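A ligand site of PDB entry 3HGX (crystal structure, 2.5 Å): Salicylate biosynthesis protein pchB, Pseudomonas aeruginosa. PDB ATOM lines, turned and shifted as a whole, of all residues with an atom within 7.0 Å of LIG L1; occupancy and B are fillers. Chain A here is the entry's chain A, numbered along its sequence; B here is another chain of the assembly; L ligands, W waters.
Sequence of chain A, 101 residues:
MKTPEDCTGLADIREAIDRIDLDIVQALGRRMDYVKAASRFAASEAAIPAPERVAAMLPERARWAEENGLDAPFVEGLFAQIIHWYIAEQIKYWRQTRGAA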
ATOM      1  N   ARG A  31       1.184 -33.179   4.120  1.00  0.00           N
ATOM      2  CA  ARG A  31       0.355 -32.924   2.948  1.00  0.00           C
ATOM      3  C   ARG A  31       1.131 -32.061   1.958  1.00  0.00           C
ATOM      4  O   ARG A  31       1.049 -32.281   0.745  1.00  0.00           O
ATOM      5  CB  ARG A  31      -0.953 -32.249   3.346  1.00  0.00           C
ATOM      6  CG  ARG A  31      -2.017 -32.224   2.254  1.00  0.00           C
ATOM      7  CD  ARG A  31      -3.123 -31.229   2.607  1.00  0.00           C
ATOM      8  NE  ARG A  31      -4.323 -31.407   1.802  1.00  0.00           N
ATOM      9  CZ  ARG A  31      -4.469 -30.963   0.554  1.00  0.00           C
ATOM     10  NH1 ARG A  31      -3.489 -30.318  -0.062  1.00  0.00           N
ATOM     11  NH2 ARG A  31      -5.612 -31.192  -0.087  1.00  0.00           N
ATOM     12  N   VAL A  35       2.001 -32.610  -2.054  1.00  0.00           N
ATOM     13  CA  VAL A  35       1.643 -31.566  -3.012  1.00  0.00           C
ATOM     14  C   VAL A  35       2.869 -31.146  -3.817  1.00  0.00           C
ATOM     15  O   VAL A  35       2.780 -30.987  -5.021  1.00  0.00           O
ATOM     16  CB  VAL A  35       0.975 -30.341  -2.292  1.00  0.00           C
ATOM     17  CG1 VAL A  35       0.896 -29.114  -3.209  1.00  0.00           C
ATOM     18  CG2 VAL A  35      -0.406 -30.724  -1.726  1.00  0.00           C
ATOM     19  N   LYS A  36       4.008 -30.997  -3.157  1.00  0.00           N
ATOM     20  CA  LYS A  36       5.249 -30.658  -3.861  1.00  0.00           C
ATOM     21  C   LYS A  36       5.692 -31.763  -4.845  1.00  0.00           C
ATOM     22  O   LYS A  36       6.100 -31.478  -5.968  1.00  0.00           O
ATOM     23  CB  LYS A  36       6.367 -30.255  -2.876  1.00  0.00           C
ATOM     24  CG  LYS A  36       6.260 -28.788  -2.414  1.00  0.00           C
ATOM     25  CD  LYS A  36       7.191 -28.425  -1.236  1.00  0.00           C
ATOM     26  CE  LYS A  36       6.944 -26.968  -0.775  1.00  0.00           C
ATOM     27  NZ  LYS A  36       7.676 -26.543   0.464  1.00  0.00           N
ATOM     28  N   ALA A  38       3.734 -33.794  -6.341  1.00  0.00           N
ATOM     29  CA  ALA A  38       2.763 -33.839  -7.446  1.00  0.00           C
ATOM     30  C   ALA A  38       3.123 -32.936  -8.621  1.00  0.00           C
ATOM     31  O   ALA A  38       2.605 -33.104  -9.715  1.00  0.00           O
ATOM     32  CB  ALA A  38       1.367 -33.518  -6.953  1.00  0.00           C
ATOM     33  N   ALA A  47      -1.607 -27.228 -16.038  1.00  0.00           N
ATOM     34  CA  ALA A  47      -2.108 -28.527 -15.599  1.00  0.00           C
ATOM     35  C   ALA A  47      -2.290 -28.640 -14.080  1.00  0.00           C
ATOM     36  O   ALA A  47      -3.019 -29.518 -13.616  1.00  0.00           O
ATOM     37  CB  ALA A  47      -1.190 -29.662 -16.118  1.00  0.00           C
ATOM     38  N   ILE A  48      -1.654 -27.749 -13.315  1.00  0.00           N
ATOM     39  CA  ILE A  48      -1.613 -27.885 -11.851  1.00  0.00           C
ATOM     40  C   ILE A  48      -2.965 -27.704 -11.100  1.00  0.00           C
ATOM     41  O   ILE A  48      -3.355 -28.583 -10.345  1.00  0.00           O
ATOM     42  CB  ILE A  48      -0.461 -27.043 -11.220  1.00  0.00           C
ATOM     43  CG1 ILE A  48       0.908 -27.604 -11.704  1.00  0.00           C
ATOM     44  CG2 ILE A  48      -0.582 -27.029  -9.684  1.00  0.00           C
ATOM     45  CD1 ILE A  48       2.144 -26.826 -11.256  1.00  0.00           C
ATOM     46  N   PRO A  49      -3.686 -26.579 -11.318  1.00  0.00           N
ATOM     47  CA  PRO A  49      -4.936 -26.351 -10.587  1.00  0.00           C
ATOM     48  C   PRO A  49      -6.004 -27.452 -10.698  1.00  0.00           C
ATOM     49  O   PRO A  49      -6.795 -27.607  -9.772  1.00  0.00           O
ATOM     50  CB  PRO A  49      -5.457 -25.039 -11.185  1.00  0.00           C
ATOM     51  CG  PRO A  49      -4.203 -24.322 -11.606  1.00  0.00           C
ATOM     52  CD  PRO A  49      -3.368 -25.434 -12.193  1.00  0.00           C
ATOM     53  N   ALA A  50      -6.014 -28.177 -11.824  1.00  0.00           N
ATOM     54  CA  ALA A  50      -6.898 -29.334 -12.030  1.00  0.00           C
ATOM     55  C   ALA A  50      -8.315 -29.213 -11.414  1.00  0.00           C
ATOM     56  O   ALA A  50      -8.652 -29.944 -10.480  1.00  0.00           O
ATOM     57  CB  ALA A  50      -6.192 -30.612 -11.548  1.00  0.00           C
ATOM     58  N   PRO A  51      -9.154 -28.311 -11.963  1.00  0.00           N
ATOM     59  CA  PRO A  51     -10.466 -27.955 -11.390  1.00  0.00           C
ATOM     60  C   PRO A  51     -11.391 -29.151 -11.200  1.00  0.00           C
ATOM     61  O   PRO A  51     -12.256 -29.152 -10.313  1.00  0.00           O
ATOM     62  CB  PRO A  51     -11.060 -27.015 -12.439  1.00  0.00           C
ATOM     63  CG  PRO A  51      -9.891 -26.441 -13.135  1.00  0.00           C
ATOM     64  CD  PRO A  51      -8.888 -27.546 -13.202  1.00  0.00           C
ATOM     65  N   ARG A  53     -10.463 -32.167 -10.297  1.00  0.00           N
ATOM     66  CA  ARG A  53     -10.064 -32.751  -9.023  1.00  0.00           C
ATOM     67  C   ARG A  53     -10.647 -31.985  -7.831  1.00  0.00           C
ATOM     68  O   ARG A  53     -11.105 -32.593  -6.870  1.00  0.00           O
ATOM     69  CB  ARG A  53      -8.542 -32.820  -8.878  1.00  0.00           C
ATOM     70  CG  ARG A  53      -8.057 -34.161  -8.375  1.00  0.00           C
ATOM     71  CD  ARG A  53      -7.835 -34.255  -6.870  1.00  0.00           C
ATOM     72  NE  ARG A  53      -8.583 -35.390  -6.359  1.00  0.00           N
ATOM     73  CZ  ARG A  53      -8.328 -36.055  -5.231  1.00  0.00           C
ATOM     74  NH1 ARG A  53      -9.118 -37.062  -4.890  1.00  0.00           N
ATOM     75  NH2 ARG A  53      -7.312 -35.721  -4.451  1.00  0.00           N
ATOM     76  N   VAL A  54     -10.634 -30.651  -7.911  1.00  0.00           N
ATOM     77  CA  VAL A  54     -11.139 -29.812  -6.811  1.00  0.00           C
ATOM     78  C   VAL A  54     -12.635 -30.065  -6.613  1.00  0.00           C
ATOM     79  O   VAL A  54     -13.091 -30.249  -5.481  1.00  0.00           O
ATOM     80  CB  VAL A  54     -10.796 -28.302  -7.030  1.00  0.00           C
ATOM     81  CG1 VAL A  54     -11.308 -27.449  -5.882  1.00  0.00           C
ATOM     82  CG2 VAL A  54      -9.272 -28.112  -7.176  1.00  0.00           C
ATOM     83  N   MET A  57     -13.189 -33.384  -4.903  1.00  0.00           N
ATOM     84  CA  MET A  57     -12.645 -33.425  -3.548  1.00  0.00           C
ATOM     85  C   MET A  57     -13.628 -32.818  -2.537  1.00  0.00           C
ATOM     86  O   MET A  57     -13.810 -33.338  -1.428  1.00  0.00           O
ATOM     87  CB  MET A  57     -11.326 -32.656  -3.471  1.00  0.00           C
ATOM     88  CG  MET A  57     -10.134 -33.381  -4.070  1.00  0.00           C
ATOM     89  SD  MET A  57      -8.629 -32.376  -4.051  1.00  0.00           S
ATOM     90  CE  MET A  57      -8.149 -32.584  -2.350  1.00  0.00           C
ATOM     91  N   ARG A  61     -15.143 -34.431   1.106  1.00  0.00           N
ATOM     92  CA  ARG A  61     -14.798 -33.913   2.426  1.00  0.00           C
ATOM     93  C   ARG A  61     -16.041 -33.471   3.210  1.00  0.00           C
ATOM     94  O   ARG A  61     -16.074 -33.566   4.430  1.00  0.00           O
ATOM     95  CB  ARG A  61     -13.803 -32.775   2.306  1.00  0.00           C
ATOM     96  CG  ARG A  61     -12.380 -33.247   2.181  1.00  0.00           C
ATOM     97  CD  ARG A  61     -11.652 -32.621   1.000  1.00  0.00           C
ATOM     98  NE  ARG A  61     -10.426 -33.363   0.776  1.00  0.00           N
ATOM     99  CZ  ARG A  61     -10.316 -34.462   0.028  1.00  0.00           C
ATOM    100  NH1 ARG A  61     -11.363 -34.947  -0.636  1.00  0.00           N
ATOM    101  NH2 ARG A  61      -9.132 -35.061  -0.063  1.00  0.00           N
ATOM    102  N   ILE A  82      -7.825 -24.488   2.053  1.00  0.00           N
ATOM    103  CA  ILE A  82      -6.615 -25.315   2.103  1.00  0.00           C
ATOM    104  C   ILE A  82      -6.143 -25.663   0.687  1.00  0.00           C
ATOM    105  O   ILE A  82      -4.969 -25.466   0.343  1.00  0.00           O
ATOM    106  CB  ILE A  82      -6.858 -26.626   2.916  1.00  0.00           C
ATOM    107  CG1 ILE A  82      -6.997 -26.319   4.405  1.00  0.00           C
ATOM    108  CG2 ILE A  82      -5.736 -27.638   2.695  1.00  0.00           C
ATOM    109  CD1 ILE A  82      -7.348 -27.518   5.268  1.00  0.00           C
ATOM    110  N   ILE A  83      -7.073 -26.152  -0.129  1.00  0.00           N
ATOM    111  CA  ILE A  83      -6.731 -26.679  -1.445  1.00  0.00           C
ATOM    112  C   ILE A  83      -6.161 -25.581  -2.337  1.00  0.00           C
ATOM    113  O   ILE A  83      -5.098 -25.760  -2.927  1.00  0.00           O
ATOM    114  CB  ILE A  83      -7.937 -27.447  -2.077  1.00  0.00           C
ATOM    115  CG1 ILE A  83      -8.226 -28.741  -1.279  1.00  0.00           C
ATOM    116  CG2 ILE A  83      -7.701 -27.739  -3.586  1.00  0.00           C
ATOM    117  CD1 ILE A  83      -9.614 -29.338  -1.507  1.00  0.00           C
ATOM    118  N   HIS A  84      -6.827 -24.430  -2.386  1.00  0.00           N
ATOM    119  CA  HIS A  84      -6.301 -23.276  -3.115  1.00  0.00           C
ATOM    120  C   HIS A  84      -4.958 -22.711  -2.598  1.00  0.00           C
ATOM    121  O   HIS A  84      -4.146 -22.260  -3.395  1.00  0.00           O
ATOM    122  CB  HIS A  84      -7.374 -22.189  -3.345  1.00  0.00           C
ATOM    123  CG  HIS A  84      -8.426 -22.606  -4.318  1.00  0.00           C
ATOM    124  ND1 HIS A  84      -9.759 -22.720  -3.974  1.00  0.00           N
ATOM    125  CD2 HIS A  84      -8.342 -22.997  -5.606  1.00  0.00           C
ATOM    126  CE1 HIS A  84     -10.446 -23.153  -5.011  1.00  0.00           C
ATOM    127  NE2 HIS A  84      -9.605 -23.330  -6.026  1.00  0.00           N
ATOM    128  N   TRP A  85      -4.720 -22.781  -1.293  1.00  0.00           N
ATOM    129  CA  TRP A  85      -3.390 -22.475  -0.771  1.00  0.00           C
ATOM    130  C   TRP A  85      -2.310 -23.414  -1.355  1.00  0.00           C
ATOM    131  O   TRP A  85      -1.231 -22.948  -1.734  1.00  0.00           O
ATOM    132  CB  TRP A  85      -3.377 -22.530   0.761  1.00  0.00           C
ATOM    133  CG  TRP A  85      -1.990 -22.366   1.371  1.00  0.00           C
ATOM    134  CD1 TRP A  85      -1.181 -23.351   1.886  1.00  0.00           C
ATOM    135  CD2 TRP A  85      -1.258 -21.145   1.510  1.00  0.00           C
ATOM    136  NE1 TRP A  85      -0.003 -22.809   2.344  1.00  0.00           N
ATOM    137  CE2 TRP A  85      -0.020 -21.455   2.121  1.00  0.00           C
ATOM    138  CE3 TRP A  85      -1.530 -19.808   1.178  1.00  0.00           C
ATOM    139  CZ2 TRP A  85       0.936 -20.480   2.408  1.00  0.00           C
ATOM    140  CZ3 TRP A  85      -0.563 -18.832   1.463  1.00  0.00           C
ATOM    141  CH2 TRP A  85       0.658 -19.170   2.064  1.00  0.00           C
ATOM    142  N   TYR A  86      -2.606 -24.718  -1.389  1.00  0.00           N
ATOM    143  CA  TYR A  86      -1.645 -25.714  -1.841  1.00  0.00           C
ATOM    144  C   TYR A  86      -1.446 -25.691  -3.351  1.00  0.00           C
ATOM    145  O   TYR A  86      -0.352 -25.962  -3.816  1.00  0.00           O
ATOM    146  CB  TYR A  86      -2.020 -27.128  -1.378  1.00  0.00           C
ATOM    147  CG  TYR A  86      -1.691 -27.392   0.063  1.00  0.00           C
ATOM    148  CD1 TYR A  86      -0.569 -28.114   0.420  1.00  0.00           C
ATOM    149  CD2 TYR A  86      -2.498 -26.904   1.086  1.00  0.00           C
ATOM    150  CE1 TYR A  86      -0.266 -28.353   1.759  1.00  0.00           C
ATOM    151  CE2 TYR A  86      -2.198 -27.137   2.413  1.00  0.00           C
ATOM    152  CZ  TYR A  86      -1.090 -27.851   2.735  1.00  0.00           C
ATOM    153  OH  TYR A  86      -0.804 -28.068   4.057  1.00  0.00           O
ATOM    154  N   ILE A  87      -2.497 -25.366  -4.103  1.00  0.00           N
ATOM    155  CA  ILE A  87      -2.350 -25.125  -5.538  1.00  0.00           C
ATOM    156  C   ILE A  87      -1.349 -23.986  -5.786  1.00  0.00           C
ATOM    157  O   ILE A  87      -0.437 -24.140  -6.590  1.00  0.00           O
ATOM    158  CB  ILE A  87      -3.691 -24.815  -6.240  1.00  0.00           C
ATOM    159  CG1 ILE A  87      -4.590 -26.050  -6.249  1.00  0.00           C
ATOM    160  CG2 ILE A  87      -3.439 -24.371  -7.686  1.00  0.00           C
ATOM    161  CD1 ILE A  87      -6.065 -25.782  -6.571  1.00  0.00           C
ATOM    162  N   ALA A  88      -1.525 -22.879  -5.069  1.00  0.00           N
ATOM    163  CA  ALA A  88      -0.624 -21.727  -5.180  1.00  0.00           C
ATOM    164  C   ALA A  88       0.807 -22.046  -4.691  1.00  0.00           C
ATOM    165  O   ALA A  88       1.770 -21.565  -5.271  1.00  0.00           O
ATOM    166  CB  ALA A  88      -1.185 -20.515  -4.439  1.00  0.00           C
ATOM    167  N   GLN A  90       2.020 -25.154  -4.796  1.00  0.00           N
ATOM    168  CA  GLN A  90       2.500 -26.091  -5.819  1.00  0.00           C
ATOM    169  C   GLN A  90       3.099 -25.394  -7.029  1.00  0.00           C
ATOM    170  O   GLN A  90       4.170 -25.766  -7.490  1.00  0.00           O
ATOM    171  CB  GLN A  90       1.402 -27.065  -6.269  1.00  0.00           C
ATOM    172  CG  GLN A  90       1.989 -28.308  -6.926  1.00  0.00           C
ATOM    173  CD  GLN A  90       0.969 -29.297  -7.438  1.00  0.00           C
ATOM    174  OE1 GLN A  90      -0.129 -29.452  -6.889  1.00  0.00           O
ATOM    175  NE2 GLN A  90       1.328 -29.999  -8.515  1.00  0.00           N
ATOM    176  N   ARG B  14      -2.795 -38.750  -4.788  1.00  0.00           N
ATOM    177  CA  ARG B  14      -4.137 -38.458  -4.319  1.00  0.00           C
ATOM    178  C   ARG B  14      -4.648 -39.490  -3.336  1.00  0.00           C
ATOM    179  O   ARG B  14      -5.495 -39.176  -2.516  1.00  0.00           O
ATOM    180  CB  ARG B  14      -5.094 -38.284  -5.489  1.00  0.00           C
ATOM    181  CG  ARG B  14      -4.797 -37.031  -6.284  1.00  0.00           C
ATOM    182  CD  ARG B  14      -5.380 -37.126  -7.665  1.00  0.00           C
ATOM    183  NE  ARG B  14      -5.187 -35.889  -8.408  1.00  0.00           N
ATOM    184  CZ  ARG B  14      -5.646 -35.682  -9.644  1.00  0.00           C
ATOM    185  NH1 ARG B  14      -5.445 -34.511 -10.237  1.00  0.00           N
ATOM    186  NH2 ARG B  14      -6.315 -36.641 -10.267  1.00  0.00           N
ATOM    187  N   ILE B  17      -3.064 -38.001  -0.089  1.00  0.00           N
ATOM    188  CA  ILE B  17      -3.695 -36.732   0.286  1.00  0.00           C
ATOM    189  C   ILE B  17      -5.112 -36.939   0.824  1.00  0.00           C
ATOM    190  O   ILE B  17      -5.505 -36.275   1.810  1.00  0.00           O
ATOM    191  CB  ILE B  17      -3.657 -35.676  -0.864  1.00  0.00           C
ATOM    192  CG1 ILE B  17      -2.227 -35.214  -1.131  1.00  0.00           C
ATOM    193  CG2 ILE B  17      -4.479 -34.430  -0.494  1.00  0.00           C
ATOM    194  CD1 ILE B  17      -2.055 -34.489  -2.459  1.00  0.00           C
ATOM    195  N   ASP B  21      -6.241 -35.858   4.473  1.00  0.00           N
ATOM    196  CA  ASP B  21      -7.421 -35.017   4.640  1.00  0.00           C
ATOM    197  C   ASP B  21      -8.460 -35.657   5.565  1.00  0.00           C
ATOM    198  O   ASP B  21      -9.095 -34.963   6.350  1.00  0.00           O
ATOM    199  CB  ASP B  21      -8.045 -34.647   3.291  1.00  0.00           C
ATOM    200  CG  ASP B  21      -7.213 -33.627   2.509  1.00  0.00           C
ATOM    201  OD1 ASP B  21      -6.201 -33.138   3.046  1.00  0.00           O
ATOM    202  OD2 ASP B  21      -7.583 -33.298   1.354  1.00  0.00           O
HETATM  203  C1  LIG L   1      -4.426 -30.371  -3.400  1.00  0.00           C
HETATM  204  O1  LIG L   1      -3.544 -29.775  -2.746  1.00  0.00           O
HETATM  205  O2  LIG L   1      -5.226 -31.153  -2.861  1.00  0.00           O
HETATM  206  C2  LIG L   1      -4.548 -30.134  -4.864  1.00  0.00           C
HETATM  207  C3  LIG L   1      -3.447 -29.437  -5.599  1.00  0.00           C
HETATM  208  C4  LIG L   1      -3.592 -29.240  -6.973  1.00  0.00           C
HETATM  209  C5  LIG L   1      -4.750 -29.668  -7.620  1.00  0.00           C
HETATM  210  C6  LIG L   1      -5.784 -30.310  -6.927  1.00  0.00           C
HETATM  211  C7  LIG L   1      -5.684 -30.542  -5.560  1.00  0.00           C
HETATM  212  O3  LIG L   1      -2.319 -29.015  -4.949  1.00  0.00           O
HETATM  213  C1  LG2 L   2      -3.645 -33.012  -7.618  1.00  0.00           C
HETATM  214  O1  LG2 L   2      -4.493 -33.617  -6.841  1.00  0.00           O
HETATM  215  O2  LG2 L   2      -3.941 -32.872  -8.870  1.00  0.00           O
HETATM  216  C2  LG2 L   2      -2.437 -32.506  -7.128  1.00  0.00           C
HETATM  217  O3  LG2 L   2      -1.629 -31.879  -7.942  1.00  0.00           O
HETATM  218  C3  LG2 L   2      -2.043 -32.681  -5.688  1.00  0.00           C
HETATM  219  O   HOH W   1      -5.419 -33.594  -4.329  1.00  0.00           O
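O1 of LIG L1 lies within salt-bridge range of NH1 of Arg 31.
NH1 of Arg 14 of chain B lies within salt-bridge range of O2 of LG2 L2.
The side-chain amide oxygen (OE1) of Gln 90 sits at hydrogen-bond distance from an oxygen (O3) of LIG L1, at 3.0 Å.
OE1 of Gln 90 lies close to O3 of LG2 L2 (3.0 Å).
O of Met 57 lies within hydrogen-bond range of NH1 of Arg 61, 3.0 Å away.
The side-chain sulfur (SD) of Met 57 lies close to the guanidinium group (NH2) of Arg 53 (3.6 Å).
The guanidinium group of Arg 31 lies within salt-bridge range of the side-chain carboxylate of Asp 21 of chain B (2.8 Å).
Merely in contact with LIG L1: Ile 48 (3.2 Å), Met 57 (3.3 Å), Tyr 86 (3.3 Å), Ile 87 (3.4 Å), Val 35 (3.4 Å), Pro 49 (3.6 Å) and Ile 83 (3.98 Å).
Hydrophobic or aromatic side chains that line LIG L1: Val 35, Met 57, Ile 83, Tyr 86 and Ile 87.
Nine residues have an atom within 4 Å of LIG L1: Arg 31, Val 35, Ile 48, Pro 49, Met 57, Ile 83, Tyr 86, Ile 87 and Gln 90.
The nearest printed residue that does not touch LIG L1 is Ile 17 of chain B (4.1 Å).
Water W1 lies within hydrogen-bond range of O1 of LG2 L2, NH2 of Arg 53, O2 of LIG L1 and SD of Met 57.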
